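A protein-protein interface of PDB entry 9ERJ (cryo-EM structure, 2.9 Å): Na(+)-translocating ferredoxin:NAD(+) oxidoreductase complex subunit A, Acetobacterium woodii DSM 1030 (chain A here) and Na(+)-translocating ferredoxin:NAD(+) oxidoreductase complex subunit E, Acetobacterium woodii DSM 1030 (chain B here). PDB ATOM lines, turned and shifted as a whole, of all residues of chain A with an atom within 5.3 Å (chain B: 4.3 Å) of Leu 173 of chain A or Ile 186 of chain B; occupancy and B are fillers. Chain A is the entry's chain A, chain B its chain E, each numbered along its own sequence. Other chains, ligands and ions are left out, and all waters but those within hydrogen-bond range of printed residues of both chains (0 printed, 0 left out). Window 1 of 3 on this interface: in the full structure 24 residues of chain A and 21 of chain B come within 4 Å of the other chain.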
ATOM      1  N   LEU A  28     -38.281  22.828  23.601  1.00  0.00           N
ATOM      2  CA  LEU A  28     -36.912  22.437  23.914  1.00  0.00           C
ATOM      3  C   LEU A  28     -36.835  21.045  24.530  1.00  0.00           C
ATOM      4  O   LEU A  28     -35.821  20.360  24.369  1.00  0.00           O
ATOM      5  CB  LEU A  28     -36.273  23.460  24.853  1.00  0.00           C
ATOM      6  CG  LEU A  28     -36.288  24.917  24.386  1.00  0.00           C
ATOM      7  CD1 LEU A  28     -35.745  25.833  25.468  1.00  0.00           C
ATOM      8  CD2 LEU A  28     -35.498  25.079  23.099  1.00  0.00           C
ATOM      9  N   PHE A 150     -37.753  21.688  14.114  1.00  0.00           N
ATOM     10  CA  PHE A 150     -36.685  21.697  15.113  1.00  0.00           C
ATOM     11  C   PHE A 150     -36.086  20.308  15.308  1.00  0.00           C
ATOM     12  O   PHE A 150     -34.855  20.153  15.379  1.00  0.00           O
ATOM     13  CB  PHE A 150     -37.218  22.236  16.440  1.00  0.00           C
ATOM     14  CG  PHE A 150     -36.160  22.813  17.333  1.00  0.00           C
ATOM     15  CD1 PHE A 150     -35.027  23.400  16.798  1.00  0.00           C
ATOM     16  CD2 PHE A 150     -36.297  22.767  18.708  1.00  0.00           C
ATOM     17  CE1 PHE A 150     -34.055  23.930  17.620  1.00  0.00           C
ATOM     18  CE2 PHE A 150     -35.328  23.296  19.533  1.00  0.00           C
ATOM     19  CZ  PHE A 150     -34.206  23.878  18.988  1.00  0.00           C
ATOM     20  N   PHE A 169     -28.520  23.026  25.533  1.00  0.00           N
ATOM     21  CA  PHE A 169     -29.472  24.137  25.553  1.00  0.00           C
ATOM     22  C   PHE A 169     -28.996  25.396  24.817  1.00  0.00           C
ATOM     23  O   PHE A 169     -29.818  26.026  24.135  1.00  0.00           O
ATOM     24  CB  PHE A 169     -29.863  24.476  26.999  1.00  0.00           C
ATOM     25  CG  PHE A 169     -30.918  23.573  27.572  1.00  0.00           C
ATOM     26  CD1 PHE A 169     -32.189  23.529  27.022  1.00  0.00           C
ATOM     27  CD2 PHE A 169     -30.643  22.774  28.668  1.00  0.00           C
ATOM     28  CE1 PHE A 169     -33.160  22.700  27.549  1.00  0.00           C
ATOM     29  CE2 PHE A 169     -31.611  21.943  29.200  1.00  0.00           C
ATOM     30  CZ  PHE A 169     -32.870  21.906  28.640  1.00  0.00           C
ATOM     31  N   PRO A 170     -27.729  25.839  24.948  1.00  0.00           N
ATOM     32  CA  PRO A 170     -27.308  27.012  24.157  1.00  0.00           C
ATOM     33  C   PRO A 170     -27.447  26.848  22.651  1.00  0.00           C
ATOM     34  O   PRO A 170     -27.903  27.783  21.977  1.00  0.00           O
ATOM     35  CB  PRO A 170     -25.840  27.199  24.559  1.00  0.00           C
ATOM     36  CG  PRO A 170     -25.722  26.615  25.890  1.00  0.00           C
ATOM     37  CD  PRO A 170     -26.782  25.577  26.053  1.00  0.00           C
ATOM     38  N   ILE A 171     -27.078  25.691  22.096  1.00  0.00           N
ATOM     39  CA  ILE A 171     -27.175  25.542  20.647  1.00  0.00           C
ATOM     40  C   ILE A 171     -28.637  25.433  20.222  1.00  0.00           C
ATOM     41  O   ILE A 171     -29.006  25.887  19.133  1.00  0.00           O
ATOM     42  CB  ILE A 171     -26.320  24.356  20.151  1.00  0.00           C
ATOM     43  CG1 ILE A 171     -25.625  24.725  18.841  1.00  0.00           C
ATOM     44  CG2 ILE A 171     -27.152  23.110  19.907  1.00  0.00           C
ATOM     45  CD1 ILE A 171     -24.640  25.859  18.972  1.00  0.00           C
ATOM     46  N   ALA A 172     -29.496  24.876  21.084  1.00  0.00           N
ATOM     47  CA  ALA A 172     -30.925  24.854  20.794  1.00  0.00           C
ATOM     48  C   ALA A 172     -31.500  26.262  20.765  1.00  0.00           C
ATOM     49  O   ALA A 172     -32.305  26.594  19.886  1.00  0.00           O
ATOM     50  CB  ALA A 172     -31.655  23.993  21.822  1.00  0.00           C
ATOM     51  N   LEU A 173     -31.087  27.111  21.709  1.00  0.00           N
ATOM     52  CA  LEU A 173     -31.574  28.487  21.727  1.00  0.00           C
ATOM     53  C   LEU A 173     -31.070  29.276  20.520  1.00  0.00           C
ATOM     54  O   LEU A 173     -31.819  30.068  19.933  1.00  0.00           O
ATOM     55  CB  LEU A 173     -31.173  29.169  23.035  1.00  0.00           C
ATOM     56  CG  LEU A 173     -31.914  28.684  24.286  1.00  0.00           C
ATOM     57  CD1 LEU A 173     -31.034  28.776  25.521  1.00  0.00           C
ATOM     58  CD2 LEU A 173     -33.203  29.459  24.493  1.00  0.00           C
ATOM     59  N   LEU A 174     -29.808  29.069  20.126  1.00  0.00           N
ATOM     60  CA  LEU A 174     -29.286  29.750  18.941  1.00  0.00           C
ATOM     61  C   LEU A 174     -30.001  29.294  17.669  1.00  0.00           C
ATOM     62  O   LEU A 174     -30.317  30.117  16.793  1.00  0.00           O
ATOM     63  CB  LEU A 174     -27.779  29.522  18.826  1.00  0.00           C
ATOM     64  CG  LEU A 174     -26.898  30.144  19.914  1.00  0.00           C
ATOM     65  CD1 LEU A 174     -25.624  29.340  20.102  1.00  0.00           C
ATOM     66  CD2 LEU A 174     -26.566  31.587  19.588  1.00  0.00           C
ATOM     67  N   THR A 175     -30.268  27.989  17.550  1.00  0.00           N
ATOM     68  CA  THR A 175     -31.034  27.482  16.416  1.00  0.00           C
ATOM     69  C   THR A 175     -32.438  28.074  16.388  1.00  0.00           C
ATOM     70  O   THR A 175     -32.945  28.442  15.319  1.00  0.00           O
ATOM     71  CB  THR A 175     -31.102  25.957  16.477  1.00  0.00           C
ATOM     72  OG1 THR A 175     -29.779  25.418  16.580  1.00  0.00           O
ATOM     73  CG2 THR A 175     -31.774  25.403  15.240  1.00  0.00           C
ATOM     74  N   ALA A 176     -33.081  28.172  17.556  1.00  0.00           N
ATOM     75  CA  ALA A 176     -34.409  28.769  17.627  1.00  0.00           C
ATOM     76  C   ALA A 176     -34.380  30.233  17.208  1.00  0.00           C
ATOM     77  O   ALA A 176     -35.307  30.712  16.549  1.00  0.00           O
ATOM     78  CB  ALA A 176     -34.976  28.621  19.036  1.00  0.00           C
ATOM     79  N   GLY A 177     -33.321  30.958  17.573  1.00  0.00           N
ATOM     80  CA  GLY A 177     -33.201  32.344  17.137  1.00  0.00           C
ATOM     81  C   GLY A 177     -33.044  32.482  15.633  1.00  0.00           C
ATOM     82  O   GLY A 177     -33.639  33.373  15.012  1.00  0.00           O
ATOM     83  N   LEU A 178     -32.240  31.607  15.023  1.00  0.00           N
ATOM     84  CA  LEU A 178     -32.088  31.651  13.568  1.00  0.00           C
ATOM     85  C   LEU A 178     -33.398  31.312  12.856  1.00  0.00           C
ATOM     86  O   LEU A 178     -33.763  31.960  11.862  1.00  0.00           O
ATOM     87  CB  LEU A 178     -30.965  30.714  13.126  1.00  0.00           C
ATOM     88  CG  LEU A 178     -29.567  31.035  13.668  1.00  0.00           C
ATOM     89  CD1 LEU A 178     -28.556  30.001  13.206  1.00  0.00           C
ATOM     90  CD2 LEU A 178     -29.128  32.433  13.263  1.00  0.00           C
ATOM     91  N   PHE B  18     -31.279  29.297  34.888  1.00  0.00           N
ATOM     92  CA  PHE B  18     -29.970  28.945  34.354  1.00  0.00           C
ATOM     93  C   PHE B  18     -29.605  27.477  34.525  1.00  0.00           C
ATOM     94  O   PHE B  18     -28.774  26.973  33.762  1.00  0.00           O
ATOM     95  CB  PHE B  18     -28.880  29.804  35.008  1.00  0.00           C
ATOM     96  CG  PHE B  18     -28.941  31.256  34.629  1.00  0.00           C
ATOM     97  CD1 PHE B  18     -28.926  31.641  33.300  1.00  0.00           C
ATOM     98  CD2 PHE B  18     -29.009  32.237  35.604  1.00  0.00           C
ATOM     99  CE1 PHE B  18     -28.982  32.978  32.949  1.00  0.00           C
ATOM    100  CE2 PHE B  18     -29.064  33.575  35.259  1.00  0.00           C
ATOM    101  CZ  PHE B  18     -29.050  33.945  33.930  1.00  0.00           C
ATOM    102  N   PHE B 179     -33.575  34.868  22.333  1.00  0.00           N
ATOM    103  CA  PHE B 179     -33.031  33.509  22.307  1.00  0.00           C
ATOM    104  C   PHE B 179     -31.511  33.510  22.334  1.00  0.00           C
ATOM    105  O   PHE B 179     -30.897  33.060  23.312  1.00  0.00           O
ATOM    106  CB  PHE B 179     -33.503  32.780  21.047  1.00  0.00           C
ATOM    107  CG  PHE B 179     -34.898  32.238  21.124  1.00  0.00           C
ATOM    108  CD1 PHE B 179     -35.221  31.230  22.014  1.00  0.00           C
ATOM    109  CD2 PHE B 179     -35.877  32.703  20.265  1.00  0.00           C
ATOM    110  CE1 PHE B 179     -36.501  30.718  22.065  1.00  0.00           C
ATOM    111  CE2 PHE B 179     -37.157  32.193  20.308  1.00  0.00           C
ATOM    112  CZ  PHE B 179     -37.470  31.202  21.211  1.00  0.00           C
ATOM    113  N   LEU B 182     -29.763  34.752  25.550  1.00  0.00           N
ATOM    114  CA  LEU B 182     -29.886  33.819  26.661  1.00  0.00           C
ATOM    115  C   LEU B 182     -28.963  32.633  26.463  1.00  0.00           C
ATOM    116  O   LEU B 182     -28.213  32.268  27.380  1.00  0.00           O
ATOM    117  CB  LEU B 182     -31.335  33.359  26.814  1.00  0.00           C
ATOM    118  CG  LEU B 182     -31.645  32.541  28.069  1.00  0.00           C
ATOM    119  CD1 LEU B 182     -31.206  33.280  29.321  1.00  0.00           C
ATOM    120  CD2 LEU B 182     -33.124  32.203  28.138  1.00  0.00           C
ATOM    121  N   GLY B 183     -28.924  32.099  25.234  1.00  0.00           N
ATOM    122  CA  GLY B 183     -28.067  30.960  24.967  1.00  0.00           C
ATOM    123  C   GLY B 183     -26.624  31.261  25.303  1.00  0.00           C
ATOM    124  O   GLY B 183     -25.991  30.519  26.064  1.00  0.00           O
ATOM    125  N   LEU B 184     -26.136  32.425  24.855  1.00  0.00           N
ATOM    126  CA  LEU B 184     -24.750  32.785  25.118  1.00  0.00           C
ATOM    127  C   LEU B 184     -24.489  32.832  26.612  1.00  0.00           C
ATOM    128  O   LEU B 184     -23.518  32.229  27.093  1.00  0.00           O
ATOM    129  CB  LEU B 184     -24.416  34.125  24.463  1.00  0.00           C
ATOM    130  CG  LEU B 184     -24.299  34.127  22.936  1.00  0.00           C
ATOM    131  CD1 LEU B 184     -24.118  35.540  22.413  1.00  0.00           C
ATOM    132  CD2 LEU B 184     -23.159  33.235  22.479  1.00  0.00           C
ATOM    133  N   LEU B 185     -25.415  33.439  27.367  1.00  0.00           N
ATOM    134  CA  LEU B 185     -25.244  33.531  28.811  1.00  0.00           C
ATOM    135  C   LEU B 185     -25.094  32.149  29.419  1.00  0.00           C
ATOM    136  O   LEU B 185     -24.122  31.888  30.143  1.00  0.00           O
ATOM    137  CB  LEU B 185     -26.423  34.271  29.440  1.00  0.00           C
ATOM    138  CG  LEU B 185     -26.407  35.796  29.341  1.00  0.00           C
ATOM    139  CD1 LEU B 185     -27.590  36.392  30.084  1.00  0.00           C
ATOM    140  CD2 LEU B 185     -25.099  36.354  29.876  1.00  0.00           C
ATOM    141  N   ILE B 186     -25.979  31.221  29.035  1.00  0.00           N
ATOM    142  CA  ILE B 186     -25.922  29.881  29.603  1.00  0.00           C
ATOM    143  C   ILE B 186     -24.584  29.243  29.280  1.00  0.00           C
ATOM    144  O   ILE B 186     -23.914  28.698  30.170  1.00  0.00           O
ATOM    145  CB  ILE B 186     -27.101  29.028  29.103  1.00  0.00           C
ATOM    146  CG1 ILE B 186     -28.425  29.605  29.605  1.00  0.00           C
ATOM    147  CG2 ILE B 186     -26.950  27.590  29.565  1.00  0.00           C
ATOM    148  CD1 ILE B 186     -29.634  28.788  29.209  1.00  0.00           C
ATOM    149  N   GLY B 187     -24.128  29.403  28.031  1.00  0.00           N
ATOM    150  CA  GLY B 187     -22.853  28.831  27.642  1.00  0.00           C
ATOM    151  C   GLY B 187     -21.728  29.324  28.525  1.00  0.00           C
ATOM    152  O   GLY B 187     -20.945  28.524  29.048  1.00  0.00           O
ATOM    153  N   LEU B 188     -21.710  30.637  28.793  1.00  0.00           N
ATOM    154  CA  LEU B 188     -20.665  31.204  29.635  1.00  0.00           C
ATOM    155  C   LEU B 188     -20.657  30.532  30.997  1.00  0.00           C
ATOM    156  O   LEU B 188     -19.608  30.055  31.452  1.00  0.00           O
ATOM    157  CB  LEU B 188     -20.863  32.712  29.774  1.00  0.00           C
ATOM    158  CG  LEU B 188     -19.782  33.485  30.527  1.00  0.00           C
ATOM    159  CD1 LEU B 188     -18.450  33.368  29.809  1.00  0.00           C
ATOM    160  CD2 LEU B 188     -20.184  34.942  30.679  1.00  0.00           C
ATOM    161  N   ILE B 189     -21.842  30.381  31.601  1.00  0.00           N
ATOM    162  CA  ILE B 189     -21.928  29.762  32.917  1.00  0.00           C
ATOM    163  C   ILE B 189     -21.364  28.354  32.862  1.00  0.00           C
ATOM    164  O   ILE B 189     -20.510  27.981  33.680  1.00  0.00           O
ATOM    165  CB  ILE B 189     -23.382  29.779  33.426  1.00  0.00           C
ATOM    166  CG1 ILE B 189     -23.780  31.194  33.847  1.00  0.00           C
ATOM    167  CG2 ILE B 189     -23.558  28.811  34.583  1.00  0.00           C
ATOM    168  CD1 ILE B 189     -25.263  31.374  34.049  1.00  0.00           C
ATOM    169  N   ASN B 190     -21.744  27.595  31.825  1.00  0.00           N
ATOM    170  CA  ASN B 190     -21.268  26.223  31.704  1.00  0.00           C
ATOM    171  C   ASN B 190     -19.752  26.192  31.633  1.00  0.00           C
ATOM    172  O   ASN B 190     -19.108  25.395  32.327  1.00  0.00           O
ATOM    173  CB  ASN B 190     -21.880  25.555  30.474  1.00  0.00           C
ATOM    174  CG  ASN B 190     -23.294  25.074  30.716  1.00  0.00           C
ATOM    175  OD1 ASN B 190     -23.901  25.385  31.739  1.00  0.00           O
ATOM    176  ND2 ASN B 190     -23.828  24.310  29.772  1.00  0.00           N
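CB of Pro 170 of chain A touches O of Gly 183 of chain B (3.6 Å). Ile 186 of chain B touches Pro 170 of chain A (CG2 to CG, 3.996 Å). Pro 170 of chain A touches Gly 187 of chain B. Leu 173 of chain A touches Phe 179 of chain B. Leu 173 of chain A touches Gly 183 of chain B. Leu 173 of chain A touches Ile 186 of chain B (CD1 to CD1, 3.9 Å). Phe 179 of chain B touches Ala 176 of chain A. CB of Phe 179 of chain B touches N of Gly 177 of chain A, at 3.9 Å.
Printed residues of chain B within 4 Å of Pro 170 of chain A: Gly 183 (3.6 Å), Ile 186 (3.996 Å) and Gly 187 (3.9 Å). Printed residues of chain B within 4 Å of Ala 176 of chain A: Phe 179. Printed residues of chain B within 4 Å of Gly 177 of chain A: Phe 179. Of the printed residues of chain A, Gly 183 of chain B touches Pro 170 and Leu 173. Of the printed residues of chain A, Ile 186 of chain B touches Pro 170 and Leu 173. Of the printed residues of chain A, Gly 187 of chain B touches Pro 170. The nearest printed residue of chain B that does not touch Leu 173 of chain A is Leu 182 of chain B (4.5 Å). The nearest printed residue of chain A that does not touch Ile 186 of chain B is Phe 169 of chain A (4.9 Å). The nearest printed residue of chain A that does not touch Phe 179 of chain B is Leu 174 of chain A (5.2 Å).
Of the 12 printed residues of chain A, 4 touch a printed residue of chain B. Among the printed residues, 8 pairs touch across the chains. Among the printed residues, no Asp or Glu carboxylate lies within 4 Å of a Lys or Arg side-chain nitrogen of the other chain.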
